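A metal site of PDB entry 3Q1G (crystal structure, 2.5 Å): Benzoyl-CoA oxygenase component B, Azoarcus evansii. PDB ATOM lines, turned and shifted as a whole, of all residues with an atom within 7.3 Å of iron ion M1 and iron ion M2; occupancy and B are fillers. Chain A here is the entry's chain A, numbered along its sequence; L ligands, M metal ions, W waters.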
ATOM      1  N   GLN A 116       1.225 -10.243  35.614  1.00  0.00           N
ATOM      2  CA  GLN A 116       1.298 -10.673  34.203  1.00  0.00           C
ATOM      3  C   GLN A 116       0.013 -10.251  33.518  1.00  0.00           C
ATOM      4  O   GLN A 116       0.047  -9.701  32.438  1.00  0.00           O
ATOM      5  CB  GLN A 116       1.518 -12.169  34.077  1.00  0.00           C
ATOM      6  CG  GLN A 116       1.597 -12.660  32.668  1.00  0.00           C
ATOM      7  CD  GLN A 116       2.747 -12.031  31.881  1.00  0.00           C
ATOM      8  OE1 GLN A 116       3.894 -12.073  32.309  1.00  0.00           O
ATOM      9  NE2 GLN A 116       2.427 -11.424  30.732  1.00  0.00           N
ATOM     10  N   THR A 119      -0.309  -6.378  32.331  1.00  0.00           N
ATOM     11  CA  THR A 119       0.438  -5.893  31.174  1.00  0.00           C
ATOM     12  C   THR A 119      -0.349  -6.094  29.865  1.00  0.00           C
ATOM     13  O   THR A 119      -0.115  -5.397  28.870  1.00  0.00           O
ATOM     14  CB  THR A 119       1.797  -6.603  30.994  1.00  0.00           C
ATOM     15  OG1 THR A 119       1.563  -7.975  30.611  1.00  0.00           O
ATOM     16  CG2 THR A 119       2.658  -6.519  32.258  1.00  0.00           C
ATOM     17  N   GLU A 120      -1.278  -7.033  29.874  1.00  0.00           N
ATOM     18  CA  GLU A 120      -1.984  -7.429  28.649  1.00  0.00           C
ATOM     19  C   GLU A 120      -2.916  -6.328  28.163  1.00  0.00           C
ATOM     20  O   GLU A 120      -2.719  -5.800  27.078  1.00  0.00           O
ATOM     21  CB  GLU A 120      -2.717  -8.768  28.823  1.00  0.00           C
ATOM     22  CG  GLU A 120      -1.856  -9.893  29.464  1.00  0.00           C
ATOM     23  CD  GLU A 120      -0.720 -10.365  28.548  1.00  0.00           C
ATOM     24  OE1 GLU A 120      -0.645  -9.913  27.391  1.00  0.00           O
ATOM     25  OE2 GLU A 120       0.061 -11.223  29.009  1.00  0.00           O
ATOM     26  N   SER A 123      -1.128  -3.033  27.160  1.00  0.00           N
ATOM     27  CA  SER A 123      -0.593  -2.869  25.793  1.00  0.00           C
ATOM     28  C   SER A 123      -1.637  -2.364  24.823  1.00  0.00           C
ATOM     29  O   SER A 123      -1.373  -1.487  23.993  1.00  0.00           O
ATOM     30  CB  SER A 123       0.070  -4.145  25.264  1.00  0.00           C
ATOM     31  OG  SER A 123      -0.861  -5.210  25.036  1.00  0.00           O
ATOM     32  N   GLN A 127      -1.779   1.258  22.738  1.00  0.00           N
ATOM     33  CA  GLN A 127      -1.750   1.195  21.268  1.00  0.00           C
ATOM     34  C   GLN A 127      -3.076   1.542  20.580  1.00  0.00           C
ATOM     35  O   GLN A 127      -3.150   1.458  19.358  1.00  0.00           O
ATOM     36  CB  GLN A 127      -1.323  -0.206  20.836  1.00  0.00           C
ATOM     37  CG  GLN A 127       0.055  -0.638  21.336  1.00  0.00           C
ATOM     38  CD  GLN A 127       0.265  -2.118  21.237  1.00  0.00           C
ATOM     39  OE1 GLN A 127       1.192  -2.666  21.825  1.00  0.00           O
ATOM     40  NE2 GLN A 127      -0.622  -2.785  20.494  1.00  0.00           N
ATOM     41  N   VAL A 146      -2.349  -8.408  16.967  1.00  0.00           N
ATOM     42  CA  VAL A 146      -1.689  -8.300  18.268  1.00  0.00           C
ATOM     43  C   VAL A 146      -2.714  -7.887  19.327  1.00  0.00           C
ATOM     44  O   VAL A 146      -2.794  -8.503  20.384  1.00  0.00           O
ATOM     45  CB  VAL A 146      -0.529  -7.301  18.264  1.00  0.00           C
ATOM     46  CG1 VAL A 146      -0.002  -7.077  19.696  1.00  0.00           C
ATOM     47  CG2 VAL A 146       0.587  -7.773  17.338  1.00  0.00           C
ATOM     48  N   GLU A 149      -5.085 -10.661  20.528  1.00  0.00           N
ATOM     49  CA  GLU A 149      -4.366 -11.701  21.244  1.00  0.00           C
ATOM     50  C   GLU A 149      -3.964 -11.243  22.640  1.00  0.00           C
ATOM     51  O   GLU A 149      -4.027 -12.007  23.609  1.00  0.00           O
ATOM     52  CB  GLU A 149      -3.165 -12.149  20.429  1.00  0.00           C
ATOM     53  CG  GLU A 149      -3.614 -12.876  19.157  1.00  0.00           C
ATOM     54  CD  GLU A 149      -2.452 -13.428  18.327  1.00  0.00           C
ATOM     55  OE1 GLU A 149      -1.286 -13.043  18.597  1.00  0.00           O
ATOM     56  OE2 GLU A 149      -2.717 -14.236  17.396  1.00  0.00           O
ATOM     57  N   GLU A 150      -3.589  -9.980  22.769  1.00  0.00           N
ATOM     58  CA  GLU A 150      -3.327  -9.453  24.127  1.00  0.00           C
ATOM     59  C   GLU A 150      -4.628  -9.488  24.961  1.00  0.00           C
ATOM     60  O   GLU A 150      -4.599  -9.775  26.154  1.00  0.00           O
ATOM     61  CB  GLU A 150      -2.670  -8.090  24.088  1.00  0.00           C
ATOM     62  CG  GLU A 150      -1.362  -8.074  23.269  1.00  0.00           C
ATOM     63  CD  GLU A 150      -0.180  -8.781  23.932  1.00  0.00           C
ATOM     64  OE1 GLU A 150      -0.364  -9.603  24.900  1.00  0.00           O
ATOM     65  OE2 GLU A 150       0.930  -8.515  23.444  1.00  0.00           O
ATOM     66  N   GLY A 151      -5.753  -9.258  24.285  1.00  0.00           N
ATOM     67  CA  GLY A 151      -7.040  -9.455  24.911  1.00  0.00           C
ATOM     68  C   GLY A 151      -7.165 -10.874  25.404  1.00  0.00           C
ATOM     69  O   GLY A 151      -7.561 -11.104  26.546  1.00  0.00           O
ATOM     70  N   HIS A 153      -4.901 -12.913  26.160  1.00  0.00           N
ATOM     71  CA  HIS A 153      -4.009 -13.134  27.277  1.00  0.00           C
ATOM     72  C   HIS A 153      -4.607 -12.656  28.569  1.00  0.00           C
ATOM     73  O   HIS A 153      -4.357 -13.269  29.586  1.00  0.00           O
ATOM     74  CB  HIS A 153      -2.660 -12.455  27.046  1.00  0.00           C
ATOM     75  CG  HIS A 153      -1.881 -13.091  25.941  1.00  0.00           C
ATOM     76  ND1 HIS A 153      -0.645 -12.639  25.530  1.00  0.00           N
ATOM     77  CD2 HIS A 153      -2.194 -14.137  25.144  1.00  0.00           C
ATOM     78  CE1 HIS A 153      -0.211 -13.413  24.552  1.00  0.00           C
ATOM     79  NE2 HIS A 153      -1.137 -14.313  24.281  1.00  0.00           N
ATOM     80  N   LEU A 154      -5.404 -11.576  28.536  1.00  0.00           N
ATOM     81  CA  LEU A 154      -6.153 -11.154  29.707  1.00  0.00           C
ATOM     82  C   LEU A 154      -7.148 -12.217  30.113  1.00  0.00           C
ATOM     83  O   LEU A 154      -7.266 -12.546  31.304  1.00  0.00           O
ATOM     84  CB  LEU A 154      -6.866  -9.834  29.458  1.00  0.00           C
ATOM     85  CG  LEU A 154      -7.629  -9.277  30.683  1.00  0.00           C
ATOM     86  CD1 LEU A 154      -6.679  -9.098  31.868  1.00  0.00           C
ATOM     87  CD2 LEU A 154      -8.333  -7.999  30.348  1.00  0.00           C
ATOM     88  N   PHE A 206       8.353  -1.741  20.526  1.00  0.00           N
ATOM     89  CA  PHE A 206       7.685  -2.302  21.675  1.00  0.00           C
ATOM     90  C   PHE A 206       7.457  -3.783  21.451  1.00  0.00           C
ATOM     91  O   PHE A 206       7.846  -4.615  22.287  1.00  0.00           O
ATOM     92  CB  PHE A 206       6.374  -1.606  21.945  1.00  0.00           C
ATOM     93  CG  PHE A 206       5.730  -2.011  23.217  1.00  0.00           C
ATOM     94  CD1 PHE A 206       5.883  -1.257  24.365  1.00  0.00           C
ATOM     95  CD2 PHE A 206       4.943  -3.169  23.266  1.00  0.00           C
ATOM     96  CE1 PHE A 206       5.281  -1.656  25.552  1.00  0.00           C
ATOM     97  CE2 PHE A 206       4.334  -3.573  24.458  1.00  0.00           C
ATOM     98  CZ  PHE A 206       4.519  -2.851  25.597  1.00  0.00           C
ATOM     99  N   THR A 207       6.852  -4.143  20.329  1.00  0.00           N
ATOM    100  CA  THR A 207       6.557  -5.529  20.110  1.00  0.00           C
ATOM    101  C   THR A 207       7.845  -6.294  19.876  1.00  0.00           C
ATOM    102  O   THR A 207       7.873  -7.512  20.060  1.00  0.00           O
ATOM    103  CB  THR A 207       5.593  -5.743  18.952  1.00  0.00           C
ATOM    104  OG1 THR A 207       6.089  -5.040  17.828  1.00  0.00           O
ATOM    105  CG2 THR A 207       4.248  -5.247  19.264  1.00  0.00           C
ATOM    106  N   THR A 210       9.705  -5.192  24.166  1.00  0.00           N
ATOM    107  CA  THR A 210       8.926  -5.329  25.381  1.00  0.00           C
ATOM    108  C   THR A 210       8.052  -6.575  25.379  1.00  0.00           C
ATOM    109  O   THR A 210       7.939  -7.245  26.405  1.00  0.00           O
ATOM    110  CB  THR A 210       8.092  -4.069  25.633  1.00  0.00           C
ATOM    111  OG1 THR A 210       8.963  -2.911  25.515  1.00  0.00           O
ATOM    112  CG2 THR A 210       7.434  -4.134  26.985  1.00  0.00           C
ATOM    113  N   ASP A 211       7.445  -6.919  24.251  1.00  0.00           N
ATOM    114  CA  ASP A 211       6.752  -8.202  24.159  1.00  0.00           C
ATOM    115  C   ASP A 211       7.768  -9.327  24.399  1.00  0.00           C
ATOM    116  O   ASP A 211       7.407 -10.417  24.856  1.00  0.00           O
ATOM    117  CB  ASP A 211       6.077  -8.375  22.796  1.00  0.00           C
ATOM    118  CG  ASP A 211       4.746  -7.618  22.678  1.00  0.00           C
ATOM    119  OD1 ASP A 211       4.714  -6.365  22.773  1.00  0.00           O
ATOM    120  OD2 ASP A 211       3.722  -8.304  22.461  1.00  0.00           O
ATOM    121  N   ARG A 212       9.048  -9.083  24.111  1.00  0.00           N
ATOM    122  CA  ARG A 212      10.056 -10.104  24.377  1.00  0.00           C
ATOM    123  C   ARG A 212      10.275 -10.344  25.868  1.00  0.00           C
ATOM    124  O   ARG A 212      10.588 -11.459  26.279  1.00  0.00           O
ATOM    125  CB  ARG A 212      11.356  -9.788  23.687  1.00  0.00           C
ATOM    126  CG  ARG A 212      12.236 -11.004  23.452  1.00  0.00           C
ATOM    127  CD  ARG A 212      13.473 -10.575  22.702  1.00  0.00           C
ATOM    128  NE  ARG A 212      13.085 -10.012  21.423  1.00  0.00           N
ATOM    129  CZ  ARG A 212      12.874 -10.729  20.320  1.00  0.00           C
ATOM    130  NH1 ARG A 212      13.043 -12.060  20.315  1.00  0.00           N
ATOM    131  NH2 ARG A 212      12.506 -10.117  19.213  1.00  0.00           N
ATOM    132  N   GLY A 214       7.782 -10.206  27.805  1.00  0.00           N
ATOM    133  CA  GLY A 214       6.663 -11.144  27.914  1.00  0.00           C
ATOM    134  C   GLY A 214       7.172 -12.553  27.664  1.00  0.00           C
ATOM    135  O   GLY A 214       6.970 -13.450  28.504  1.00  0.00           O
ATOM    136  N   LYS A 215       7.857 -12.764  26.533  1.00  0.00           N
ATOM    137  CA  LYS A 215       8.344 -14.093  26.180  1.00  0.00           C
ATOM    138  C   LYS A 215       9.049 -14.692  27.392  1.00  0.00           C
ATOM    139  O   LYS A 215       8.723 -15.808  27.852  1.00  0.00           O
ATOM    140  CB  LYS A 215       9.291 -14.039  24.963  1.00  0.00           C
ATOM    141  CG  LYS A 215       9.972 -15.398  24.577  1.00  0.00           C
ATOM    142  CD  LYS A 215      11.029 -15.195  23.505  1.00  0.00           C
ATOM    143  CE  LYS A 215      11.759 -16.473  23.119  1.00  0.00           C
ATOM    144  NZ  LYS A 215      12.676 -16.224  21.908  1.00  0.00           N
ATOM    145  N   LEU A 218       6.992 -15.327  30.635  1.00  0.00           N
ATOM    146  CA  LEU A 218       6.099 -16.453  30.371  1.00  0.00           C
ATOM    147  C   LEU A 218       6.848 -17.785  30.283  1.00  0.00           C
ATOM    148  O   LEU A 218       6.361 -18.785  30.777  1.00  0.00           O
ATOM    149  CB  LEU A 218       5.340 -16.231  29.056  1.00  0.00           C
ATOM    150  CG  LEU A 218       4.292 -15.125  29.047  1.00  0.00           C
ATOM    151  CD1 LEU A 218       3.828 -14.869  27.599  1.00  0.00           C
ATOM    152  CD2 LEU A 218       3.097 -15.416  29.978  1.00  0.00           C
ATOM    153  N   MET A 236       0.565 -19.402  25.440  1.00  0.00           N
ATOM    154  CA  MET A 236       0.750 -17.998  25.225  1.00  0.00           C
ATOM    155  C   MET A 236       2.046 -17.728  24.469  1.00  0.00           C
ATOM    156  O   MET A 236       2.077 -16.837  23.633  1.00  0.00           O
ATOM    157  CB  MET A 236       0.709 -17.238  26.543  1.00  0.00           C
ATOM    158  CG  MET A 236      -0.673 -17.188  27.152  1.00  0.00           C
ATOM    159  SD  MET A 236      -0.734 -16.570  28.825  1.00  0.00           S
ATOM    160  CE  MET A 236      -0.140 -14.896  28.526  1.00  0.00           C
ATOM    161  N   GLU A 239       1.645 -17.456  20.849  1.00  0.00           N
ATOM    162  CA  GLU A 239       1.099 -16.166  20.471  1.00  0.00           C
ATOM    163  C   GLU A 239       2.169 -15.067  20.531  1.00  0.00           C
ATOM    164  O   GLU A 239       2.283 -14.235  19.622  1.00  0.00           O
ATOM    165  CB  GLU A 239      -0.090 -15.816  21.351  1.00  0.00           C
ATOM    166  CG  GLU A 239      -1.295 -16.731  21.073  1.00  0.00           C
ATOM    167  CD  GLU A 239      -2.330 -16.742  22.190  1.00  0.00           C
ATOM    168  OE1 GLU A 239      -1.971 -16.770  23.386  1.00  0.00           O
ATOM    169  OE2 GLU A 239      -3.533 -16.755  21.856  1.00  0.00           O
ATOM    170  N   GLU A 240       2.981 -15.096  21.588  1.00  0.00           N
ATOM    171  CA  GLU A 240       4.017 -14.088  21.713  1.00  0.00           C
ATOM    172  C   GLU A 240       4.974 -14.151  20.529  1.00  0.00           C
ATOM    173  O   GLU A 240       5.492 -13.115  20.114  1.00  0.00           O
ATOM    174  CB  GLU A 240       4.784 -14.222  23.010  1.00  0.00           C
ATOM    175  CG  GLU A 240       5.384 -12.880  23.446  1.00  0.00           C
ATOM    176  CD  GLU A 240       4.315 -11.875  23.964  1.00  0.00           C
ATOM    177  OE1 GLU A 240       3.813 -11.043  23.218  1.00  0.00           O
ATOM    178  OE2 GLU A 240       3.981 -11.874  25.130  1.00  0.00           O
ATOM    179  N   ALA A 241       5.208 -15.349  19.972  1.00  0.00           N
ATOM    180  CA  ALA A 241       6.060 -15.476  18.787  1.00  0.00           C
ATOM    181  C   ALA A 241       5.587 -14.583  17.642  1.00  0.00           C
ATOM    182  O   ALA A 241       6.396 -14.007  16.952  1.00  0.00           O
ATOM    183  CB  ALA A 241       6.172 -16.938  18.322  1.00  0.00           C
ATOM    184  N   HIS A 242       4.274 -14.466  17.450  1.00  0.00           N
ATOM    185  CA  HIS A 242       3.726 -13.607  16.393  1.00  0.00           C
ATOM    186  C   HIS A 242       4.004 -12.137  16.666  1.00  0.00           C
ATOM    187  O   HIS A 242       4.276 -11.375  15.728  1.00  0.00           O
ATOM    188  CB  HIS A 242       2.206 -13.780  16.183  1.00  0.00           C
ATOM    189  CG  HIS A 242       1.642 -12.906  15.092  1.00  0.00           C
ATOM    190  ND1 HIS A 242       1.778 -13.189  13.743  1.00  0.00           N
ATOM    191  CD2 HIS A 242       0.950 -11.731  15.150  1.00  0.00           C
ATOM    192  CE1 HIS A 242       1.194 -12.243  13.021  1.00  0.00           C
ATOM    193  NE2 HIS A 242       0.683 -11.354  13.846  1.00  0.00           N
ATOM    194  N   HIS A 243       3.964 -11.745  17.920  1.00  0.00           N
ATOM    195  CA  HIS A 243       4.129 -10.357  18.296  1.00  0.00           C
ATOM    196  C   HIS A 243       5.559  -9.931  18.026  1.00  0.00           C
ATOM    197  O   HIS A 243       5.807  -8.845  17.486  1.00  0.00           O
ATOM    198  CB  HIS A 243       3.758 -10.149  19.783  1.00  0.00           C
ATOM    199  CG  HIS A 243       2.345 -10.563  20.123  1.00  0.00           C
ATOM    200  ND1 HIS A 243       1.818 -10.456  21.399  1.00  0.00           N
ATOM    201  CD2 HIS A 243       1.357 -11.068  19.341  1.00  0.00           C
ATOM    202  CE1 HIS A 243       0.568 -10.898  21.388  1.00  0.00           C
ATOM    203  NE2 HIS A 243       0.263 -11.272  20.153  1.00  0.00           N
ATOM    204  N   LEU A 244       6.503 -10.796  18.379  1.00  0.00           N
ATOM    205  CA  LEU A 244       7.922 -10.533  18.145  1.00  0.00           C
ATOM    206  C   LEU A 244       8.179 -10.443  16.647  1.00  0.00           C
ATOM    207  O   LEU A 244       8.964  -9.593  16.197  1.00  0.00           O
ATOM    208  CB  LEU A 244       8.799 -11.629  18.730  1.00  0.00           C
ATOM    209  CG  LEU A 244       8.572 -11.914  20.221  1.00  0.00           C
ATOM    210  CD1 LEU A 244       9.450 -13.134  20.647  1.00  0.00           C
ATOM    211  CD2 LEU A 244       8.835 -10.640  21.077  1.00  0.00           C
HETATM  212  O1  LIG L   1       1.510 -11.094  24.163  1.00  0.00           O
HETATM  213 FE    FE M   1       0.758 -10.773  25.991  1.00  0.00          FE
HETATM  214 FE    FE M   2       2.585  -9.615  23.258  1.00  0.00          FE
HETATM  215  O   HOH W   1       2.732  -8.772  25.589  1.00  0.00           O
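The backbone NH (N) of Asp 211 sits at hydrogen-bond distance from the backbone carbonyl oxygen (O) of Phe 206, 3.1 Å away. The side-chain amide nitrogen (NE2) of Gln 116 sits at hydrogen-bond distance from the side-chain carboxylate (OE2) of Glu 120. O of Glu 120 lies within hydrogen-bond range of OG of Ser 123, at 2.8 Å. A ring nitrogen (NE2) of His 243 lies within hydrogen-bond range of the side-chain carboxylate (OE1) of Glu 149 (2.8 Å). OE1 of Glu 239 is in hydrogen-bond range of NE2 of His 153.
Of the 26 residues printed, 4 come within 4 Å of iron ion M2. The nearest printed residue that does not touch iron ion M2 is His 153 (4.9 Å).
Iron ion M1 is bound by OE1 of Glu 150 (2.0 Å), O1 of the ligand (2.0 Å), OE1 of Glu 120 (2.2 Å) and ND1 of His 153 (2.4 Å). Iron ion M1 has four donor atoms within binding distance. Slightly farther from iron ion M1 lies water W1 (2.8 Å).
Iron ion M2 is bound by the side-chain carboxylate of Glu 240 (1.9 Å), the side-chain carboxylate of Asp 211 (1.9 Å), the side-chain carboxylate of Glu 150 (2.0 Å), an oxygen (O1) of the ligand (2.0 Å), a ring nitrogen (ND1) of His 243 (2.2 Å) and water W1 (2.5 Å).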
